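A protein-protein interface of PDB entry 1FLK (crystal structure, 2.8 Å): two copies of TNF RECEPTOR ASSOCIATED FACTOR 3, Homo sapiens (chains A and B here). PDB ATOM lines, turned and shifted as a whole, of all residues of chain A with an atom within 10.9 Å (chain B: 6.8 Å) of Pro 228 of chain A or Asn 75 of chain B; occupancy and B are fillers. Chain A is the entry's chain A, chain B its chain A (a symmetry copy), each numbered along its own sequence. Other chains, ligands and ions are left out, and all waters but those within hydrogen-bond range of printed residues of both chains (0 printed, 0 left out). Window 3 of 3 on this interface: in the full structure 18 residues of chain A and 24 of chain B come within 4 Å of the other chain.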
ATOM      1  N   TYR A  74      -1.899 -21.530  -5.940  1.00  0.00           N
ATOM      2  CA  TYR A  74      -1.065 -21.830  -4.785  1.00  0.00           C
ATOM      3  C   TYR A  74       0.228 -21.046  -4.738  1.00  0.00           C
ATOM      4  O   TYR A  74       1.191 -21.478  -4.107  1.00  0.00           O
ATOM      5  CB  TYR A  74      -0.759 -23.336  -4.731  1.00  0.00           C
ATOM      6  CG  TYR A  74      -2.004 -24.203  -4.788  1.00  0.00           C
ATOM      7  CD1 TYR A  74      -2.568 -24.558  -6.006  1.00  0.00           C
ATOM      8  CD2 TYR A  74      -2.692 -24.560  -3.621  1.00  0.00           C
ATOM      9  CE1 TYR A  74      -3.789 -25.227  -6.067  1.00  0.00           C
ATOM     10  CE2 TYR A  74      -3.917 -25.230  -3.676  1.00  0.00           C
ATOM     11  CZ  TYR A  74      -4.460 -25.552  -4.906  1.00  0.00           C
ATOM     12  OH  TYR A  74      -5.698 -26.154  -4.993  1.00  0.00           O
ATOM     13  N   ASN A  75       0.260 -19.886  -5.387  1.00  0.00           N
ATOM     14  CA  ASN A  75       1.478 -19.073  -5.377  1.00  0.00           C
ATOM     15  C   ASN A  75       1.262 -17.719  -4.708  1.00  0.00           C
ATOM     16  O   ASN A  75       2.054 -16.804  -4.899  1.00  0.00           O
ATOM     17  CB  ASN A  75       1.977 -18.843  -6.799  1.00  0.00           C
ATOM     18  CG  ASN A  75       0.999 -18.046  -7.624  1.00  0.00           C
ATOM     19  OD1 ASN A  75       1.332 -16.987  -8.146  1.00  0.00           O
ATOM     20  ND2 ASN A  75      -0.227 -18.550  -7.741  1.00  0.00           N
ATOM     21  N   THR A 107      -0.829 -19.270  -0.435  1.00  0.00           N
ATOM     22  CA  THR A 107       0.504 -18.680  -0.582  1.00  0.00           C
ATOM     23  C   THR A 107       1.435 -19.848  -0.916  1.00  0.00           C
ATOM     24  O   THR A 107       2.536 -19.666  -1.432  1.00  0.00           O
ATOM     25  CB  THR A 107       1.004 -18.036   0.750  1.00  0.00           C
ATOM     26  OG1 THR A 107       0.921 -19.003   1.803  1.00  0.00           O
ATOM     27  CG2 THR A 107       0.167 -16.806   1.132  1.00  0.00           C
ATOM     28  N   GLY A 108       0.965 -21.052  -0.605  1.00  0.00           N
ATOM     29  CA  GLY A 108       1.729 -22.257  -0.852  1.00  0.00           C
ATOM     30  C   GLY A 108       0.811 -23.458  -0.794  1.00  0.00           C
ATOM     31  O   GLY A 108      -0.377 -23.314  -0.492  1.00  0.00           O
ATOM     32  N   TYR A 109       1.351 -24.642  -1.076  1.00  0.00           N
ATOM     33  CA  TYR A 109       0.542 -25.858  -1.068  1.00  0.00           C
ATOM     34  C   TYR A 109      -0.069 -26.168   0.295  1.00  0.00           C
ATOM     35  O   TYR A 109      -1.175 -26.730   0.379  1.00  0.00           O
ATOM     36  CB  TYR A 109       1.367 -27.053  -1.578  1.00  0.00           C
ATOM     37  CG  TYR A 109       1.309 -27.199  -3.085  1.00  0.00           C
ATOM     38  CD1 TYR A 109       2.452 -27.051  -3.870  1.00  0.00           C
ATOM     39  CD2 TYR A 109       0.093 -27.433  -3.730  1.00  0.00           C
ATOM     40  CE1 TYR A 109       2.386 -27.124  -5.270  1.00  0.00           C
ATOM     41  CE2 TYR A 109       0.013 -27.506  -5.122  1.00  0.00           C
ATOM     42  CZ  TYR A 109       1.162 -27.348  -5.891  1.00  0.00           C
ATOM     43  OH  TYR A 109       1.069 -27.393  -7.272  1.00  0.00           O
ATOM     44  N   PHE A 110       0.643 -25.787   1.355  1.00  0.00           N
ATOM     45  CA  PHE A 110       0.185 -26.012   2.722  1.00  0.00           C
ATOM     46  C   PHE A 110       0.284 -24.699   3.537  1.00  0.00           C
ATOM     47  O   PHE A 110       0.403 -24.715   4.770  1.00  0.00           O
ATOM     48  CB  PHE A 110       1.042 -27.110   3.388  1.00  0.00           C
ATOM     49  CG  PHE A 110       0.958 -28.463   2.722  1.00  0.00           C
ATOM     50  CD1 PHE A 110       2.091 -29.055   2.185  1.00  0.00           C
ATOM     51  CD2 PHE A 110      -0.251 -29.146   2.637  1.00  0.00           C
ATOM     52  CE1 PHE A 110       2.020 -30.311   1.565  1.00  0.00           C
ATOM     53  CE2 PHE A 110      -0.333 -30.405   2.021  1.00  0.00           C
ATOM     54  CZ  PHE A 110       0.803 -30.987   1.483  1.00  0.00           C
ATOM     55  N   GLY A 111       0.220 -23.569   2.838  1.00  0.00           N
ATOM     56  CA  GLY A 111       0.329 -22.275   3.492  1.00  0.00           C
ATOM     57  C   GLY A 111      -0.985 -21.629   3.898  1.00  0.00           C
ATOM     58  O   GLY A 111      -2.021 -22.304   3.978  1.00  0.00           O
ATOM     59  N   TYR A 142      -4.460 -26.486   7.586  1.00  0.00           N
ATOM     60  CA  TYR A 142      -3.090 -26.600   8.062  1.00  0.00           C
ATOM     61  C   TYR A 142      -2.673 -25.538   9.062  1.00  0.00           C
ATOM     62  O   TYR A 142      -1.477 -25.291   9.235  1.00  0.00           O
ATOM     63  CB  TYR A 142      -2.134 -26.602   6.852  1.00  0.00           C
ATOM     64  CG  TYR A 142      -2.287 -27.869   6.045  1.00  0.00           C
ATOM     65  CD1 TYR A 142      -3.499 -28.173   5.421  1.00  0.00           C
ATOM     66  CD2 TYR A 142      -1.291 -28.843   6.056  1.00  0.00           C
ATOM     67  CE1 TYR A 142      -3.724 -29.417   4.854  1.00  0.00           C
ATOM     68  CE2 TYR A 142      -1.500 -30.090   5.492  1.00  0.00           C
ATOM     69  CZ  TYR A 142      -2.721 -30.377   4.897  1.00  0.00           C
ATOM     70  OH  TYR A 142      -2.945 -31.639   4.383  1.00  0.00           O
ATOM     71  N   PRO A 147       3.086 -19.439  10.998  1.00  0.00           N
ATOM     72  CA  PRO A 147       3.416 -18.263  11.822  1.00  0.00           C
ATOM     73  C   PRO A 147       2.273 -17.222  11.979  1.00  0.00           C
ATOM     74  O   PRO A 147       1.537 -16.949  11.030  1.00  0.00           O
ATOM     75  CB  PRO A 147       4.621 -17.659  11.092  1.00  0.00           C
ATOM     76  CG  PRO A 147       5.202 -18.828  10.336  1.00  0.00           C
ATOM     77  CD  PRO A 147       3.973 -19.503   9.824  1.00  0.00           C
ATOM     78  N   THR A 222       4.519 -13.480  -0.754  1.00  0.00           N
ATOM     79  CA  THR A 222       4.918 -14.783  -0.250  1.00  0.00           C
ATOM     80  C   THR A 222       6.412 -14.925  -0.520  1.00  0.00           C
ATOM     81  O   THR A 222       7.109 -15.699   0.133  1.00  0.00           O
ATOM     82  CB  THR A 222       4.148 -15.902  -0.956  1.00  0.00           C
ATOM     83  OG1 THR A 222       4.453 -15.878  -2.352  1.00  0.00           O
ATOM     84  CG2 THR A 222       2.659 -15.706  -0.776  1.00  0.00           C
ATOM     85  N   SER A 223       6.891 -14.151  -1.489  1.00  0.00           N
ATOM     86  CA  SER A 223       8.300 -14.145  -1.864  1.00  0.00           C
ATOM     87  C   SER A 223       9.164 -13.944  -0.630  1.00  0.00           C
ATOM     88  O   SER A 223      10.071 -14.731  -0.361  1.00  0.00           O
ATOM     89  CB  SER A 223       8.577 -13.015  -2.860  1.00  0.00           C
ATOM     90  OG  SER A 223       9.967 -12.839  -3.061  1.00  0.00           O
ATOM     91  N   ASP A 224       8.880 -12.879   0.115  1.00  0.00           N
ATOM     92  CA  ASP A 224       9.636 -12.583   1.324  1.00  0.00           C
ATOM     93  C   ASP A 224       9.231 -13.522   2.448  1.00  0.00           C
ATOM     94  O   ASP A 224       8.934 -13.116   3.573  1.00  0.00           O
ATOM     95  CB  ASP A 224       9.445 -11.121   1.714  1.00  0.00           C
ATOM     96  CG  ASP A 224       9.950 -10.178   0.644  1.00  0.00           C
ATOM     97  OD1 ASP A 224       9.325 -10.134  -0.436  1.00  0.00           O
ATOM     98  OD2 ASP A 224      10.978  -9.500   0.874  1.00  0.00           O
ATOM     99  N   LEU A 225       9.225 -14.799   2.091  1.00  0.00           N
ATOM    100  CA  LEU A 225       8.902 -15.898   2.982  1.00  0.00           C
ATOM    101  C   LEU A 225       9.339 -17.151   2.213  1.00  0.00           C
ATOM    102  O   LEU A 225       8.517 -18.005   1.869  1.00  0.00           O
ATOM    103  CB  LEU A 225       7.400 -15.928   3.281  1.00  0.00           C
ATOM    104  CG  LEU A 225       7.033 -16.705   4.548  1.00  0.00           C
ATOM    105  CD1 LEU A 225       7.047 -18.189   4.276  1.00  0.00           C
ATOM    106  CD2 LEU A 225       8.019 -16.347   5.666  1.00  0.00           C
ATOM    107  N   PRO A 226      10.656 -17.263   1.935  1.00  0.00           N
ATOM    108  CA  PRO A 226      11.249 -18.385   1.204  1.00  0.00           C
ATOM    109  C   PRO A 226      10.327 -19.587   1.070  1.00  0.00           C
ATOM    110  O   PRO A 226      10.085 -20.320   2.029  1.00  0.00           O
ATOM    111  CB  PRO A 226      12.503 -18.677   2.012  1.00  0.00           C
ATOM    112  CG  PRO A 226      12.987 -17.285   2.311  1.00  0.00           C
ATOM    113  CD  PRO A 226      11.706 -16.515   2.658  1.00  0.00           C
ATOM    114  N   ASP A 227       9.802 -19.767  -0.135  1.00  0.00           N
ATOM    115  CA  ASP A 227       8.901 -20.874  -0.423  1.00  0.00           C
ATOM    116  C   ASP A 227       9.728 -22.050  -0.972  1.00  0.00           C
ATOM    117  O   ASP A 227      10.207 -22.009  -2.109  1.00  0.00           O
ATOM    118  CB  ASP A 227       7.848 -20.418  -1.439  1.00  0.00           C
ATOM    119  CG  ASP A 227       6.556 -21.194  -1.332  1.00  0.00           C
ATOM    120  OD1 ASP A 227       6.541 -22.388  -1.701  1.00  0.00           O
ATOM    121  OD2 ASP A 227       5.558 -20.604  -0.871  1.00  0.00           O
ATOM    122  N   PRO A 228       9.909 -23.108  -0.157  1.00  0.00           N
ATOM    123  CA  PRO A 228      10.670 -24.319  -0.493  1.00  0.00           C
ATOM    124  C   PRO A 228      10.612 -24.780  -1.956  1.00  0.00           C
ATOM    125  O   PRO A 228      11.693 -24.921  -2.571  1.00  0.00           O
ATOM    126  CB  PRO A 228      10.090 -25.349   0.473  1.00  0.00           C
ATOM    127  CG  PRO A 228       9.884 -24.528   1.708  1.00  0.00           C
ATOM    128  CD  PRO A 228       9.252 -23.261   1.158  1.00  0.00           C
ATOM    129  OXT PRO A 228       9.492 -25.005  -2.461  1.00  0.00           O
ATOM    130  N   ALA B  72      -2.878 -32.828  -2.055  1.00  0.00           N
ATOM    131  CA  ALA B  72      -1.657 -33.253  -2.751  1.00  0.00           C
ATOM    132  C   ALA B  72      -0.666 -32.108  -3.032  1.00  0.00           C
ATOM    133  O   ALA B  72      -1.064 -31.022  -3.429  1.00  0.00           O
ATOM    134  CB  ALA B  72      -2.026 -33.940  -4.050  1.00  0.00           C
ATOM    135  N   SER B  73       0.624 -32.356  -2.825  1.00  0.00           N
ATOM    136  CA  SER B  73       1.659 -31.350  -3.062  1.00  0.00           C
ATOM    137  C   SER B  73       2.591 -31.784  -4.194  1.00  0.00           C
ATOM    138  O   SER B  73       2.944 -32.959  -4.301  1.00  0.00           O
ATOM    139  CB  SER B  73       2.465 -31.103  -1.786  1.00  0.00           C
ATOM    140  OG  SER B  73       2.821 -32.324  -1.154  1.00  0.00           O
ATOM    141  N   TYR B  74       2.998 -30.831  -5.031  1.00  0.00           N
ATOM    142  CA  TYR B  74       3.851 -31.138  -6.169  1.00  0.00           C
ATOM    143  C   TYR B  74       5.222 -30.503  -6.102  1.00  0.00           C
ATOM    144  O   TYR B  74       5.866 -30.309  -7.131  1.00  0.00           O
ATOM    145  CB  TYR B  74       3.154 -30.727  -7.477  1.00  0.00           C
ATOM    146  CG  TYR B  74       1.760 -31.309  -7.622  1.00  0.00           C
ATOM    147  CD1 TYR B  74       0.661 -30.670  -7.063  1.00  0.00           C
ATOM    148  CD2 TYR B  74       1.558 -32.566  -8.208  1.00  0.00           C
ATOM    149  CE1 TYR B  74      -0.597 -31.269  -7.064  1.00  0.00           C
ATOM    150  CE2 TYR B  74       0.298 -33.171  -8.210  1.00  0.00           C
ATOM    151  CZ  TYR B  74      -0.771 -32.517  -7.628  1.00  0.00           C
ATOM    152  OH  TYR B  74      -2.011 -33.117  -7.558  1.00  0.00           O
ATOM    153  N   ASN B  75       5.689 -30.190  -4.897  1.00  0.00           N
ATOM    154  CA  ASN B  75       7.014 -29.580  -4.759  1.00  0.00           C
ATOM    155  C   ASN B  75       7.975 -30.460  -3.964  1.00  0.00           C
ATOM    156  O   ASN B  75       8.991 -29.980  -3.479  1.00  0.00           O
ATOM    157  CB  ASN B  75       6.906 -28.225  -4.068  1.00  0.00           C
ATOM    158  CG  ASN B  75       6.397 -28.344  -2.654  1.00  0.00           C
ATOM    159  OD1 ASN B  75       7.057 -27.923  -1.711  1.00  0.00           O
ATOM    160  ND2 ASN B  75       5.214 -28.933  -2.498  1.00  0.00           N
ATOM    161  N   GLY B  76       7.656 -31.744  -3.835  1.00  0.00           N
ATOM    162  CA  GLY B  76       8.523 -32.643  -3.093  1.00  0.00           C
ATOM    163  C   GLY B  76       8.249 -32.677  -1.591  1.00  0.00           C
ATOM    164  O   GLY B  76       8.540 -33.682  -0.926  1.00  0.00           O
ATOM    165  N   VAL B  77       7.696 -31.586  -1.052  1.00  0.00           N
ATOM    166  CA  VAL B  77       7.386 -31.507   0.370  1.00  0.00           C
ATOM    167  C   VAL B  77       5.995 -32.061   0.616  1.00  0.00           C
ATOM    168  O   VAL B  77       5.198 -32.190  -0.302  1.00  0.00           O
ATOM    169  CB  VAL B  77       7.441 -30.051   0.881  1.00  0.00           C
ATOM    170  CG1 VAL B  77       7.187 -30.004   2.386  1.00  0.00           C
ATOM    171  CG2 VAL B  77       8.789 -29.451   0.564  1.00  0.00           C
ATOM    172  N   LEU B  78       5.706 -32.392   1.866  1.00  0.00           N
ATOM    173  CA  LEU B  78       4.403 -32.940   2.224  1.00  0.00           C
ATOM    174  C   LEU B  78       4.098 -32.784   3.723  1.00  0.00           C
ATOM    175  O   LEU B  78       4.963 -33.010   4.579  1.00  0.00           O
ATOM    176  CB  LEU B  78       4.340 -34.423   1.810  1.00  0.00           C
ATOM    177  CG  LEU B  78       3.173 -35.365   2.163  1.00  0.00           C
ATOM    178  CD1 LEU B  78       3.389 -36.019   3.527  1.00  0.00           C
ATOM    179  CD2 LEU B  78       1.860 -34.598   2.106  1.00  0.00           C
ATOM    180  N   PHE B 105       1.888 -37.781  -2.994  1.00  0.00           N
ATOM    181  CA  PHE B 105       2.491 -36.483  -3.256  1.00  0.00           C
ATOM    182  C   PHE B 105       3.657 -36.649  -4.245  1.00  0.00           C
ATOM    183  O   PHE B 105       4.072 -37.777  -4.531  1.00  0.00           O
ATOM    184  CB  PHE B 105       2.906 -35.776  -1.947  1.00  0.00           C
ATOM    185  CG  PHE B 105       4.151 -36.319  -1.297  1.00  0.00           C
ATOM    186  CD1 PHE B 105       4.149 -37.561  -0.671  1.00  0.00           C
ATOM    187  CD2 PHE B 105       5.322 -35.554  -1.274  1.00  0.00           C
ATOM    188  CE1 PHE B 105       5.298 -38.033  -0.025  1.00  0.00           C
ATOM    189  CE2 PHE B 105       6.469 -36.012  -0.636  1.00  0.00           C
ATOM    190  CZ  PHE B 105       6.460 -37.253  -0.009  1.00  0.00           C
ATOM    191  N   TYR B 106       4.165 -35.543  -4.786  1.00  0.00           N
ATOM    192  CA  TYR B 106       5.223 -35.617  -5.788  1.00  0.00           C
ATOM    193  C   TYR B 106       6.391 -34.659  -5.566  1.00  0.00           C
ATOM    194  O   TYR B 106       6.403 -33.875  -4.614  1.00  0.00           O
ATOM    195  CB  TYR B 106       4.624 -35.358  -7.186  1.00  0.00           C
ATOM    196  CG  TYR B 106       3.384 -36.167  -7.477  1.00  0.00           C
ATOM    197  CD1 TYR B 106       2.218 -35.968  -6.758  1.00  0.00           C
ATOM    198  CD2 TYR B 106       3.406 -37.197  -8.393  1.00  0.00           C
ATOM    199  CE1 TYR B 106       1.112 -36.785  -6.929  1.00  0.00           C
ATOM    200  CE2 TYR B 106       2.302 -38.025  -8.578  1.00  0.00           C
ATOM    201  CZ  TYR B 106       1.161 -37.816  -7.837  1.00  0.00           C
ATOM    202  OH  TYR B 106       0.087 -38.668  -7.963  1.00  0.00           O
ATOM    203  N   THR B 107       7.371 -34.751  -6.466  1.00  0.00           N
ATOM    204  CA  THR B 107       8.571 -33.911  -6.467  1.00  0.00           C
ATOM    205  C   THR B 107       8.343 -32.872  -7.568  1.00  0.00           C
ATOM    206  O   THR B 107       8.985 -31.824  -7.607  1.00  0.00           O
ATOM    207  CB  THR B 107       9.851 -34.726  -6.835  1.00  0.00           C
ATOM    208  OG1 THR B 107       9.634 -35.412  -8.074  1.00  0.00           O
ATOM    209  CG2 THR B 107      10.198 -35.752  -5.747  1.00  0.00           C
ATOM    210  N   GLY B 108       7.416 -33.193  -8.465  1.00  0.00           N
ATOM    211  CA  GLY B 108       7.089 -32.319  -9.571  1.00  0.00           C
ATOM    212  C   GLY B 108       5.756 -32.727 -10.162  1.00  0.00           C
ATOM    213  O   GLY B 108       5.169 -33.723  -9.731  1.00  0.00           O
ATOM    214  N   TYR B 109       5.277 -31.970 -11.146  1.00  0.00           N
ATOM    215  CA  TYR B 109       3.990 -32.268 -11.766  1.00  0.00           C
ATOM    216  C   TYR B 109       3.948 -33.635 -12.444  1.00  0.00           C
ATOM    217  O   TYR B 109       2.892 -34.291 -12.480  1.00  0.00           O
ATOM    218  CB  TYR B 109       3.602 -31.158 -12.758  1.00  0.00           C
ATOM    219  CG  TYR B 109       2.853 -30.021 -12.095  1.00  0.00           C
ATOM    220  CD1 TYR B 109       3.391 -28.735 -12.041  1.00  0.00           C
ATOM    221  CD2 TYR B 109       1.625 -30.247 -11.469  1.00  0.00           C
ATOM    222  CE1 TYR B 109       2.726 -27.696 -11.371  1.00  0.00           C
ATOM    223  CE2 TYR B 109       0.954 -29.223 -10.799  1.00  0.00           C
ATOM    224  CZ  TYR B 109       1.508 -27.947 -10.748  1.00  0.00           C
ATOM    225  OH  TYR B 109       0.850 -26.945 -10.055  1.00  0.00           O
ATOM    226  N   VAL B 220      11.453 -34.784   0.758  1.00  0.00           N
ATOM    227  CA  VAL B 220      12.249 -35.422  -0.283  1.00  0.00           C
ATOM    228  C   VAL B 220      12.909 -34.322  -1.102  1.00  0.00           C
ATOM    229  O   VAL B 220      12.213 -33.515  -1.715  1.00  0.00           O
ATOM    230  CB  VAL B 220      11.352 -36.234  -1.236  1.00  0.00           C
ATOM    231  CG1 VAL B 220      12.204 -37.050  -2.186  1.00  0.00           C
ATOM    232  CG2 VAL B 220      10.406 -37.111  -0.439  1.00  0.00           C
ATOM    233  N   ASP B 221      14.239 -34.285  -1.121  1.00  0.00           N
ATOM    234  CA  ASP B 221      14.937 -33.259  -1.884  1.00  0.00           C
ATOM    235  C   ASP B 221      14.592 -33.341  -3.363  1.00  0.00           C
ATOM    236  O   ASP B 221      14.500 -34.427  -3.939  1.00  0.00           O
ATOM    237  CB  ASP B 221      16.447 -33.389  -1.732  1.00  0.00           C
ATOM    238  CG  ASP B 221      17.199 -32.409  -2.618  1.00  0.00           C
ATOM    239  OD1 ASP B 221      17.101 -31.192  -2.371  1.00  0.00           O
ATOM    240  OD2 ASP B 221      17.879 -32.848  -3.569  1.00  0.00           O
ATOM    241  N   THR B 222      14.398 -32.180  -3.969  1.00  0.00           N
ATOM    242  CA  THR B 222      14.074 -32.088  -5.383  1.00  0.00           C
ATOM    243  C   THR B 222      14.882 -30.925  -5.949  1.00  0.00           C
ATOM    244  O   THR B 222      15.145 -30.854  -7.148  1.00  0.00           O
ATOM    245  CB  THR B 222      12.577 -31.835  -5.585  1.00  0.00           C
ATOM    246  OG1 THR B 222      12.223 -30.585  -4.991  1.00  0.00           O
ATOM    247  CG2 THR B 222      11.768 -32.935  -4.935  1.00  0.00           C
ATOM    248  N   SER B 223      15.281 -30.023  -5.058  1.00  0.00           N
ATOM    249  CA  SER B 223      16.080 -28.860  -5.426  1.00  0.00           C
ATOM    250  C   SER B 223      17.293 -29.296  -6.230  1.00  0.00           C
ATOM    251  O   SER B 223      17.532 -28.799  -7.330  1.00  0.00           O
ATOM    252  CB  SER B 223      16.550 -28.124  -4.168  1.00  0.00           C
ATOM    253  OG  SER B 223      17.512 -27.134  -4.482  1.00  0.00           O
ATOM    254  N   ASP B 227      14.351 -28.264 -11.214  1.00  0.00           N
ATOM    255  CA  ASP B 227      12.946 -28.414 -11.566  1.00  0.00           C
ATOM    256  C   ASP B 227      12.556 -27.275 -12.524  1.00  0.00           C
ATOM    257  O   ASP B 227      12.436 -26.117 -12.115  1.00  0.00           O
ATOM    258  CB  ASP B 227      12.099 -28.376 -10.288  1.00  0.00           C
ATOM    259  CG  ASP B 227      10.796 -29.127 -10.427  1.00  0.00           C
ATOM    260  OD1 ASP B 227       9.901 -28.648 -11.156  1.00  0.00           O
ATOM    261  OD2 ASP B 227      10.676 -30.204  -9.809  1.00  0.00           O
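OH of Tyr 109 of chain B is in hydrogen-bond range of OH of Tyr 109 of chain A, at 2.8 Å.
O of Val 77 of chain B is in hydrogen-bond range of OG of Ser 73 of chain B (2.5 Å).
The backbone NH (N) of Tyr 106 of chain B is in hydrogen-bond range of the backbone carbonyl oxygen (O) of Ser 73 of chain B, 2.9 Å away.
Among the printed residues, merely in contact across the chains: Tyr 109 of chain A with Ala 72 of chain B (3.8 Å), Tyr 109 of chain A with Tyr 74 of chain B (3.3 Å), Tyr 109 of chain A with Asn 75 of chain B (3.6 Å), Phe 110 of chain A with Ser 73 of chain B (3.5 Å), Phe 110 of chain A with Leu 78 of chain B (3.6 Å) and Pro 228 of chain A with Asn 75 of chain B (3.9 Å).
Printed residues of chain B within 4 Å of Tyr 109 of chain A: Ala 72 (3.8 Å), Tyr 74 (3.3 Å), Asn 75 (3.6 Å) and Tyr 109 (2.8 Å).
Of the printed residues of chain B, Phe 110 of chain A touches Ser 73 (3.5 Å) and Leu 78 (3.6 Å).
Of chain B, only Asn 75 (3.9 Å) comes within 4 Å of Pro 228 of chain A.
Printed residues of chain A within 4 Å of Tyr 74 of chain B: Tyr 109.
Printed residues of chain A within 4 Å of Asn 75 of chain B: Tyr 109 and Pro 228.
No residue of chain A comes within 4 Å of Gly 76 of chain B.
No residue of chain A comes within 4 Å of Val 77 of chain B.
Of the printed residues of chain A, Leu 78 of chain B touches Phe 110.
No residue of chain A comes within 4 Å of Thr 107 of chain B.
Of the printed residues of chain A, Tyr 109 of chain B touches Tyr 109 (2.8 Å).
The nearest residue of chain A that does not touch Asn 75 of chain B is Phe 110 of chain A (5.3 Å).
The nearest printed residue of chain A that does not touch Ala 72 of chain B is Phe 110 of chain A (4.9 Å).
Hydrophobic or aromatic side chains of chain A within 4 Å of the printed part of chain B: Tyr 109 and Phe 110.
Of the 17 printed residues of chain B, 6 touch a printed residue of chain A.
Printed residues of chain B that touch a printed residue of chain A: Ala 72, Ser 73, Tyr 74, Asn 75, Leu 78 and Tyr 109.
Hydrophobic or aromatic side chains of chain B that line the printed part of chain A: Tyr 74, Leu 78 and Tyr 109.
Among the printed residues, no Asp or Glu carboxylate lies within 4 Å of a Lys or Arg side-chain nitrogen of the other chain.
Tyr 109 of chain A touches Tyr 74 of chain B, but with the chains exchanged Tyr 74 of chain A does not touch Tyr 109 of chain B (5.8 Å).
Tyr 109 of chain A touches Asn 75 of chain B, but with the chains exchanged Asn 75 of chain A does not touch Tyr 109 of chain B (8.5 Å).
Tyr 109 of chain A touches its own counterpart, Tyr 109 of chain B.
Positions printed for both chains: 74, 75, 107, 108, 109, 222, 223 and 227.
Of the 7 pairs that touch across the chains among the printed residues, 1 has its exchanged pair printed and touching as well.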
